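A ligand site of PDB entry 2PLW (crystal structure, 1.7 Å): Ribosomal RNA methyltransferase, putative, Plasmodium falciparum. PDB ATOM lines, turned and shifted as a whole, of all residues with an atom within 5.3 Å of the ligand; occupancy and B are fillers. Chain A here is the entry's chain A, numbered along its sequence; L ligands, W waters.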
ATOM      1  N   SER A   4       1.872 -34.831 -19.227  1.00  0.00           N
ATOM      2  CA  SER A   4       0.451 -35.070 -19.478  1.00  0.00           C
ATOM      3  C   SER A   4       0.283 -35.331 -20.956  1.00  0.00           C
ATOM      4  O   SER A   4       1.047 -34.843 -21.779  1.00  0.00           O
ATOM      5  CB  SER A   4      -0.422 -33.849 -19.090  1.00  0.00           C
ATOM      6  OG  SER A   4      -1.738 -33.973 -19.626  1.00  0.00           O
ATOM      7  N   ALA A   6      -2.080 -34.087 -22.496  1.00  0.00           N
ATOM      8  CA  ALA A   6      -2.535 -32.759 -23.011  1.00  0.00           C
ATOM      9  C   ALA A   6      -1.526 -32.108 -23.997  1.00  0.00           C
ATOM     10  O   ALA A   6      -1.936 -31.344 -24.889  1.00  0.00           O
ATOM     11  CB  ALA A   6      -2.842 -31.805 -21.854  1.00  0.00           C
ATOM     12  N   ALA A   7      -0.236 -32.418 -23.839  1.00  0.00           N
ATOM     13  CA  ALA A   7       0.803 -31.957 -24.782  1.00  0.00           C
ATOM     14  C   ALA A   7       0.381 -32.130 -26.229  1.00  0.00           C
ATOM     15  O   ALA A   7       0.636 -31.273 -27.053  1.00  0.00           O
ATOM     16  CB  ALA A   7       2.153 -32.692 -24.541  1.00  0.00           C
ATOM     17  N   ASP A  28       1.266 -19.469 -20.564  1.00  0.00           N
ATOM     18  CA  ASP A  28       0.503 -20.706 -20.607  1.00  0.00           C
ATOM     19  C   ASP A  28      -0.357 -20.730 -19.361  1.00  0.00           C
ATOM     20  O   ASP A  28       0.176 -20.932 -18.262  1.00  0.00           O
ATOM     21  CB  ASP A  28       1.498 -21.867 -20.605  1.00  0.00           C
ATOM     22  CG  ASP A  28       0.830 -23.230 -20.578  1.00  0.00           C
ATOM     23  OD1 ASP A  28      -0.305 -23.350 -21.064  1.00  0.00           O
ATOM     24  OD2 ASP A  28       1.448 -24.176 -20.025  1.00  0.00           O
ATOM     25  N   ILE A  29      -1.644 -20.460 -19.534  1.00  0.00           N
ATOM     26  CA  ILE A  29      -2.559 -20.364 -18.393  1.00  0.00           C
ATOM     27  C   ILE A  29      -3.179 -21.723 -18.151  1.00  0.00           C
ATOM     28  O   ILE A  29      -3.549 -22.429 -19.107  1.00  0.00           O
ATOM     29  CB  ILE A  29      -3.664 -19.325 -18.658  1.00  0.00           C
ATOM     30  CG1 ILE A  29      -3.035 -17.952 -18.916  1.00  0.00           C
ATOM     31  CG2 ILE A  29      -4.667 -19.284 -17.452  1.00  0.00           C
ATOM     32  CD1 ILE A  29      -4.053 -16.870 -19.218  1.00  0.00           C
ATOM     33  N   GLY A  30      -3.286 -22.097 -16.872  1.00  0.00           N
ATOM     34  CA  GLY A  30      -3.725 -23.444 -16.496  1.00  0.00           C
ATOM     35  C   GLY A  30      -2.633 -24.449 -16.831  1.00  0.00           C
ATOM     36  O   GLY A  30      -2.891 -25.438 -17.482  1.00  0.00           O
ATOM     37  N   CYS A  31      -1.398 -24.180 -16.392  1.00  0.00           N
ATOM     38  CA  CYS A  31      -0.235 -24.910 -16.922  1.00  0.00           C
ATOM     39  C   CYS A  31       0.016 -26.257 -16.245  1.00  0.00           C
ATOM     40  O   CYS A  31       0.806 -27.046 -16.778  1.00  0.00           O
ATOM     41  CB  CYS A  31       1.059 -24.083 -16.847  1.00  0.00           C
ATOM     42  SG  CYS A  31       1.495 -23.564 -15.182  1.00  0.00           S
ATOM     43  N   TYR A  32      -0.605 -26.507 -15.083  1.00  0.00           N
ATOM     44  CA  TYR A  32      -0.326 -27.743 -14.318  1.00  0.00           C
ATOM     45  C   TYR A  32      -0.799 -28.977 -15.063  1.00  0.00           C
ATOM     46  O   TYR A  32      -1.937 -28.994 -15.550  1.00  0.00           O
ATOM     47  CB  TYR A  32      -0.995 -27.694 -12.951  1.00  0.00           C
ATOM     48  CG  TYR A  32      -0.711 -28.916 -12.113  1.00  0.00           C
ATOM     49  CD1 TYR A  32       0.262 -28.887 -11.151  1.00  0.00           C
ATOM     50  CD2 TYR A  32      -1.425 -30.109 -12.321  1.00  0.00           C
ATOM     51  CE1 TYR A  32       0.572 -30.027 -10.400  1.00  0.00           C
ATOM     52  CE2 TYR A  32      -1.142 -31.257 -11.592  1.00  0.00           C
ATOM     53  CZ  TYR A  32      -0.149 -31.205 -10.638  1.00  0.00           C
ATOM     54  OH  TYR A  32       0.145 -32.326  -9.886  1.00  0.00           O
ATOM     55  N   PRO A  33       0.016 -30.046 -15.097  1.00  0.00           N
ATOM     56  CA  PRO A  33       1.339 -30.268 -14.476  1.00  0.00           C
ATOM     57  C   PRO A  33       2.513 -29.764 -15.283  1.00  0.00           C
ATOM     58  O   PRO A  33       3.625 -29.821 -14.779  1.00  0.00           O
ATOM     59  CB  PRO A  33       1.428 -31.808 -14.403  1.00  0.00           C
ATOM     60  CG  PRO A  33       0.675 -32.245 -15.561  1.00  0.00           C
ATOM     61  CD  PRO A  33      -0.472 -31.274 -15.748  1.00  0.00           C
ATOM     62  N   GLY A  34       2.281 -29.369 -16.526  1.00  0.00           N
ATOM     63  CA  GLY A  34       3.301 -28.638 -17.280  1.00  0.00           C
ATOM     64  C   GLY A  34       3.640 -29.078 -18.676  1.00  0.00           C
ATOM     65  O   GLY A  34       4.615 -28.593 -19.221  1.00  0.00           O
ATOM     66  N   SER A  35       2.810 -29.923 -19.295  1.00  0.00           N
ATOM     67  CA  SER A  35       3.180 -30.437 -20.610  1.00  0.00           C
ATOM     68  C   SER A  35       3.105 -29.430 -21.750  1.00  0.00           C
ATOM     69  O   SER A  35       3.865 -29.546 -22.710  1.00  0.00           O
ATOM     70  CB  SER A  35       2.413 -31.742 -20.966  1.00  0.00           C
ATOM     71  OG  SER A  35       1.090 -31.470 -21.387  1.00  0.00           O
ATOM     72  N   TRP A  36       2.225 -28.433 -21.674  1.00  0.00           N
ATOM     73  CA  TRP A  36       2.216 -27.374 -22.694  1.00  0.00           C
ATOM     74  C   TRP A  36       3.500 -26.591 -22.590  1.00  0.00           C
ATOM     75  O   TRP A  36       4.077 -26.186 -23.595  1.00  0.00           O
ATOM     76  CB  TRP A  36       0.976 -26.456 -22.533  1.00  0.00           C
ATOM     77  CG  TRP A  36      -0.256 -27.042 -23.186  1.00  0.00           C
ATOM     78  CD1 TRP A  36      -0.532 -28.393 -23.420  1.00  0.00           C
ATOM     79  CD2 TRP A  36      -1.382 -26.326 -23.735  1.00  0.00           C
ATOM     80  NE1 TRP A  36      -1.740 -28.525 -24.079  1.00  0.00           N
ATOM     81  CE2 TRP A  36      -2.274 -27.279 -24.285  1.00  0.00           C
ATOM     82  CE3 TRP A  36      -1.707 -24.951 -23.830  1.00  0.00           C
ATOM     83  CZ2 TRP A  36      -3.491 -26.933 -24.886  1.00  0.00           C
ATOM     84  CZ3 TRP A  36      -2.903 -24.602 -24.463  1.00  0.00           C
ATOM     85  CH2 TRP A  36      -3.780 -25.582 -24.977  1.00  0.00           C
ATOM     86  N   ILE A  54       1.068 -20.222 -15.625  1.00  0.00           N
ATOM     87  CA  ILE A  54       0.264 -19.802 -14.473  1.00  0.00           C
ATOM     88  C   ILE A  54      -0.701 -20.931 -14.155  1.00  0.00           C
ATOM     89  O   ILE A  54      -1.360 -21.423 -15.053  1.00  0.00           O
ATOM     90  CB  ILE A  54      -0.531 -18.512 -14.741  1.00  0.00           C
ATOM     91  CG1 ILE A  54       0.415 -17.303 -14.766  1.00  0.00           C
ATOM     92  CG2 ILE A  54      -1.535 -18.260 -13.549  1.00  0.00           C
ATOM     93  CD1 ILE A  54      -0.278 -16.004 -15.153  1.00  0.00           C
ATOM     94  N   ASP A  55      -0.799 -21.325 -12.889  1.00  0.00           N
ATOM     95  CA  ASP A  55      -1.897 -22.235 -12.489  1.00  0.00           C
ATOM     96  C   ASP A  55      -2.214 -21.997 -11.036  1.00  0.00           C
ATOM     97  O   ASP A  55      -1.348 -21.573 -10.284  1.00  0.00           O
ATOM     98  CB  ASP A  55      -1.487 -23.700 -12.672  1.00  0.00           C
ATOM     99  CG  ASP A  55      -2.653 -24.642 -12.743  1.00  0.00           C
ATOM    100  OD1 ASP A  55      -3.363 -24.836 -11.740  1.00  0.00           O
ATOM    101  OD2 ASP A  55      -2.864 -25.215 -13.818  1.00  0.00           O
ATOM    102  N   LYS A  56      -3.454 -22.273 -10.635  1.00  0.00           N
ATOM    103  CA  LYS A  56      -3.790 -22.191  -9.195  1.00  0.00           C
ATOM    104  C   LYS A  56      -3.095 -23.311  -8.411  1.00  0.00           C
ATOM    105  O   LYS A  56      -2.839 -23.160  -7.234  1.00  0.00           O
ATOM    106  CB  LYS A  56      -5.307 -22.172  -8.967  1.00  0.00           C
ATOM    107  CG  LYS A  56      -6.038 -23.390  -9.476  1.00  0.00           C
ATOM    108  CD  LYS A  56      -7.556 -23.149  -9.696  1.00  0.00           C
ATOM    109  CE  LYS A  56      -8.284 -22.902  -8.380  1.00  0.00           C
ATOM    110  NZ  LYS A  56      -9.768 -22.945  -8.593  1.00  0.00           N
ATOM    111  N   LYS A  57      -2.772 -24.414  -9.094  1.00  0.00           N
ATOM    112  CA  LYS A  57      -2.004 -25.523  -8.513  1.00  0.00           C
ATOM    113  C   LYS A  57      -0.489 -25.360  -8.742  1.00  0.00           C
ATOM    114  O   LYS A  57      -0.055 -24.979  -9.838  1.00  0.00           O
ATOM    115  CB  LYS A  57      -2.440 -26.854  -9.111  1.00  0.00           C
ATOM    116  CG  LYS A  57      -3.843 -27.317  -8.745  1.00  0.00           C
ATOM    117  CD  LYS A  57      -4.069 -28.764  -9.248  1.00  0.00           C
ATOM    118  CE  LYS A  57      -4.806 -28.748 -10.609  1.00  0.00           C
ATOM    119  NZ  LYS A  57      -4.598 -29.944 -11.513  1.00  0.00           N
ATOM    120  N   GLY A  70      -1.306 -18.848  -9.217  1.00  0.00           N
ATOM    121  CA  GLY A  70      -2.413 -17.887  -9.140  1.00  0.00           C
ATOM    122  C   GLY A  70      -3.643 -18.308  -9.898  1.00  0.00           C
ATOM    123  O   GLY A  70      -3.568 -19.026 -10.876  1.00  0.00           O
ATOM    124  N   GLU A  71      -4.800 -17.872  -9.417  1.00  0.00           N
ATOM    125  CA  GLU A  71      -6.030 -18.156 -10.112  1.00  0.00           C
ATOM    126  C   GLU A  71      -6.440 -16.933 -10.926  1.00  0.00           C
ATOM    127  O   GLU A  71      -6.754 -15.874 -10.355  1.00  0.00           O
ATOM    128  CB  GLU A  71      -7.124 -18.547  -9.098  1.00  0.00           C
ATOM    129  CG  GLU A  71      -8.488 -18.762  -9.747  1.00  0.00           C
ATOM    130  CD  GLU A  71      -9.530 -19.245  -8.740  1.00  0.00           C
ATOM    131  OE1 GLU A  71      -9.250 -19.239  -7.529  1.00  0.00           O
ATOM    132  OE2 GLU A  71     -10.631 -19.611  -9.181  1.00  0.00           O
ATOM    133  N   ILE A  72      -6.402 -17.037 -12.252  1.00  0.00           N
ATOM    134  CA  ILE A  72      -6.825 -15.899 -13.065  1.00  0.00           C
ATOM    135  C   ILE A  72      -8.298 -15.608 -12.793  1.00  0.00           C
ATOM    136  O   ILE A  72      -9.108 -16.523 -12.685  1.00  0.00           O
ATOM    137  CB  ILE A  72      -6.525 -16.139 -14.575  1.00  0.00           C
ATOM    138  CG1 ILE A  72      -5.020 -16.309 -14.762  1.00  0.00           C
ATOM    139  CG2 ILE A  72      -7.104 -15.005 -15.412  1.00  0.00           C
ATOM    140  CD1 ILE A  72      -4.163 -15.060 -14.434  1.00  0.00           C
ATOM    141  N   GLY A  73      -8.640 -14.335 -12.627  1.00  0.00           N
ATOM    142  CA  GLY A  73      -9.983 -13.974 -12.209  1.00  0.00           C
ATOM    143  C   GLY A  73     -10.074 -13.729 -10.711  1.00  0.00           C
ATOM    144  O   GLY A  73     -11.102 -13.281 -10.214  1.00  0.00           O
ATOM    145  N   ASP A 113      -5.333 -23.520 -21.385  1.00  0.00           N
ATOM    146  CA  ASP A 113      -5.917 -24.857 -21.322  1.00  0.00           C
ATOM    147  C   ASP A 113      -6.693 -25.015 -20.015  1.00  0.00           C
ATOM    148  O   ASP A 113      -6.988 -26.153 -19.595  1.00  0.00           O
ATOM    149  CB  ASP A 113      -4.810 -25.917 -21.422  1.00  0.00           C
ATOM    150  CG  ASP A 113      -5.340 -27.304 -21.747  1.00  0.00           C
ATOM    151  OD1 ASP A 113      -6.316 -27.391 -22.530  1.00  0.00           O
ATOM    152  OD2 ASP A 113      -4.757 -28.297 -21.235  1.00  0.00           O
ATOM    153  N   ALA A 114      -7.052 -23.905 -19.352  1.00  0.00           N
ATOM    154  CA  ALA A 114      -7.764 -23.971 -18.064  1.00  0.00           C
ATOM    155  C   ALA A 114      -9.209 -24.462 -18.254  1.00  0.00           C
ATOM    156  O   ALA A 114      -9.799 -24.269 -19.315  1.00  0.00           O
ATOM    157  CB  ALA A 114      -7.785 -22.596 -17.372  1.00  0.00           C
ATOM    158  N   ALA A 115      -9.748 -25.088 -17.225  1.00  0.00           N
ATOM    159  CA  ALA A 115     -11.152 -25.502 -17.221  1.00  0.00           C
ATOM    160  C   ALA A 115     -11.681 -25.492 -15.781  1.00  0.00           C
ATOM    161  O   ALA A 115     -10.907 -25.607 -14.834  1.00  0.00           O
ATOM    162  CB  ALA A 115     -11.314 -26.897 -17.857  1.00  0.00           C
ATOM    163  N   VAL A 116     -12.982 -25.294 -15.639  1.00  0.00           N
ATOM    164  CA  VAL A 116     -13.616 -25.323 -14.321  1.00  0.00           C
ATOM    165  C   VAL A 116     -14.162 -26.740 -14.096  1.00  0.00           C
ATOM    166  O   VAL A 116     -14.643 -27.344 -15.049  1.00  0.00           O
ATOM    167  CB  VAL A 116     -14.716 -24.241 -14.185  1.00  0.00           C
ATOM    168  CG1 VAL A 116     -14.115 -22.962 -13.614  1.00  0.00           C
ATOM    169  CG2 VAL A 116     -15.375 -23.931 -15.528  1.00  0.00           C
ATOM    170  N   LEU A 132     -15.382 -18.387 -16.818  1.00  0.00           N
ATOM    171  CA  LEU A 132     -13.930 -18.540 -16.768  1.00  0.00           C
ATOM    172  C   LEU A 132     -13.297 -17.949 -18.009  1.00  0.00           C
ATOM    173  O   LEU A 132     -12.269 -17.256 -17.930  1.00  0.00           O
ATOM    174  CB  LEU A 132     -13.541 -20.011 -16.620  1.00  0.00           C
ATOM    175  CG  LEU A 132     -12.026 -20.299 -16.623  1.00  0.00           C
ATOM    176  CD1 LEU A 132     -11.309 -19.471 -15.552  1.00  0.00           C
ATOM    177  CD2 LEU A 132     -11.787 -21.761 -16.394  1.00  0.00           C
ATOM    178  N   LYS A 153      -9.384 -22.389 -24.264  1.00  0.00           N
ATOM    179  CA  LYS A 153     -10.323 -23.519 -24.261  1.00  0.00           C
ATOM    180  C   LYS A 153     -11.654 -23.159 -23.588  1.00  0.00           C
ATOM    181  O   LYS A 153     -11.691 -22.378 -22.642  1.00  0.00           O
ATOM    182  CB  LYS A 153      -9.680 -24.734 -23.577  1.00  0.00           C
ATOM    183  CG  LYS A 153     -10.480 -26.036 -23.741  1.00  0.00           C
ATOM    184  CD  LYS A 153      -9.723 -27.216 -23.119  1.00  0.00           C
ATOM    185  CE  LYS A 153      -9.508 -27.162 -21.632  1.00  0.00           C
ATOM    186  NZ  LYS A 153      -8.657 -28.312 -21.195  1.00  0.00           N
HETATM  187  N1  LIG L   1      -2.205 -27.748 -20.294  1.00  0.00           N
HETATM  188  C1  LIG L   1      -1.797 -28.458 -19.040  1.00  0.00           C
HETATM  189  C2  LIG L   1      -0.628 -29.417 -19.294  1.00  0.00           C
HETATM  190  O1  LIG L   1      -0.350 -29.726 -20.459  1.00  0.00           O
HETATM  191  O2  LIG L   1       0.082 -29.872 -18.387  1.00  0.00           O
HETATM  192  C3  LIG L   1      -2.998 -29.219 -18.468  1.00  0.00           C
HETATM  193  C4  LIG L   1      -3.987 -28.197 -17.914  1.00  0.00           C
HETATM  194  S1  LIG L   1      -5.277 -28.876 -16.842  1.00  0.00           S
HETATM  195  C5  LIG L   1      -6.235 -29.742 -18.090  1.00  0.00           C
HETATM  196  C6  LIG L   1      -6.308 -27.432 -16.510  1.00  0.00           C
HETATM  197  C7  LIG L   1      -5.688 -26.549 -15.423  1.00  0.00           C
HETATM  198  O3  LIG L   1      -6.416 -25.318 -15.380  1.00  0.00           O
HETATM  199  C8  LIG L   1      -5.713 -27.125 -13.990  1.00  0.00           C
HETATM  200  O4  LIG L   1      -4.420 -27.431 -13.537  1.00  0.00           O
HETATM  201  C9  LIG L   1      -6.361 -26.020 -13.152  1.00  0.00           C
HETATM  202  O5  LIG L   1      -5.798 -25.779 -11.864  1.00  0.00           O
HETATM  203  C10 LIG L   1      -6.216 -24.812 -14.067  1.00  0.00           C
HETATM  204  N2  LIG L   1      -7.136 -23.701 -13.816  1.00  0.00           N
HETATM  205  C11 LIG L   1      -8.512 -23.714 -13.771  1.00  0.00           C
HETATM  206  N3  LIG L   1      -8.956 -22.453 -13.562  1.00  0.00           N
HETATM  207  C12 LIG L   1      -7.865 -21.647 -13.478  1.00  0.00           C
HETATM  208  C13 LIG L   1      -7.702 -20.277 -13.282  1.00  0.00           C
HETATM  209  N4  LIG L   1      -8.746 -19.471 -13.128  1.00  0.00           N
HETATM  210  N5  LIG L   1      -6.452 -19.722 -13.250  1.00  0.00           N
HETATM  211  C14 LIG L   1      -5.323 -20.509 -13.419  1.00  0.00           C
HETATM  212  N6  LIG L   1      -5.468 -21.868 -13.628  1.00  0.00           N
HETATM  213  C15 LIG L   1      -6.721 -22.415 -13.642  1.00  0.00           C
HETATM  214  O   HOH W   1      -7.073 -26.722  -9.640  1.00  0.00           O
HETATM  215  O   HOH W   2     -11.404 -20.008 -11.768  1.00  0.00           O
HETATM  216  O   HOH W   3      -6.164 -30.457 -21.228  1.00  0.00           O
HETATM  217  O   HOH W   4      -1.695 -25.066 -20.111  1.00  0.00           O
HETATM  218  O   HOH W   5       1.470 -26.751 -19.285  1.00  0.00           O
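N of Trp 36 is in hydrogen-bond range of O1 of the ligand, 3.1 Å away. N of Ile 72 lies within hydrogen-bond range of N5 of the ligand (2.9 Å). O4 of the ligand lies within hydrogen-bond range of NZ of Lys 57, 3.2 Å away. N of Gly 34 sits at hydrogen-bond distance from O2 of the ligand, at 2.9 Å. N4 of the ligand lies within hydrogen-bond range of O of Ile 72 (3.0 Å). The side-chain hydroxyl (OG) of Ser 35 sits at hydrogen-bond distance from an oxygen (O1) of the ligand (2.4 Å). The side-chain carboxylate (OD1) of Asp 55 is in hydrogen-bond range of an oxygen (O5) of the ligand (2.6 Å). The backbone NH of Ser 35 lies within hydrogen-bond range of an oxygen (O2) of the ligand. The side-chain carboxylate of Asp 113 lies within salt-bridge range of a nitrogen (N1) of the ligand.
OG of Ser 4 lies within hydrogen-bond range of N of Ala 6. OG of Ser 35 is in hydrogen-bond range of N of Ala 7 (2.9 Å). OD2 of Asp 55 is in hydrogen-bond range of N of Tyr 32, at 2.9 Å. The side-chain amino group of Lys 153 is in salt-bridge range of the side-chain carboxylate of Asp 113, at 2.8 Å. The backbone NH of Gly 30 lies within hydrogen-bond range of the backbone carbonyl oxygen of Ile 54 (2.7 Å). O of Ser 4 sits at hydrogen-bond distance from OG of Ser 35 (3.4 Å). The indole nitrogen of Trp 36 sits at hydrogen-bond distance from the backbone carbonyl oxygen of Ala 6 (2.9 Å). The side-chain carboxylate of Asp 55 sits at hydrogen-bond distance from the backbone NH of Cys 31, 3.1 Å away.
O of Cys 31 sits close to O2 of the ligand (3.3 Å). S1 of the ligand lies close to O of Tyr 32 (3.6 Å). The backbone nitrogen of Pro 33 sits close to an oxygen (O2) of the ligand (3.3 Å). Residues that only touch the ligand: Gly 30, Ala 115, Ala 114, Lys 56, Gly 70, Glu 71, Leu 132 and Ala 6. Hydrophobic or aromatic side chains within 4 Å of the ligand: Ala 6, Tyr 32, Pro 33, Trp 36, Ile 72, Ala 114 and Leu 132. The nearest printed residue that does not touch the ligand is Ser 4 (4.1 Å).
Water W2 lies within hydrogen-bond range of OE2 of Glu 71 (2.7 Å) and N4 of the ligand (3.0 Å). Water W3 bridges the side-chain carboxylate (OD2) of Asp 113 (2.6 Å) and the side-chain amino group (NZ) of Lys 153 (3.3 Å). Water W5 lies within hydrogen-bond range of O of Cys 31 (2.6 Å), OD2 of Asp 28 (2.7 Å), N of Trp 36 (3.0 Å) and N of Ser 35 (3.4 Å).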
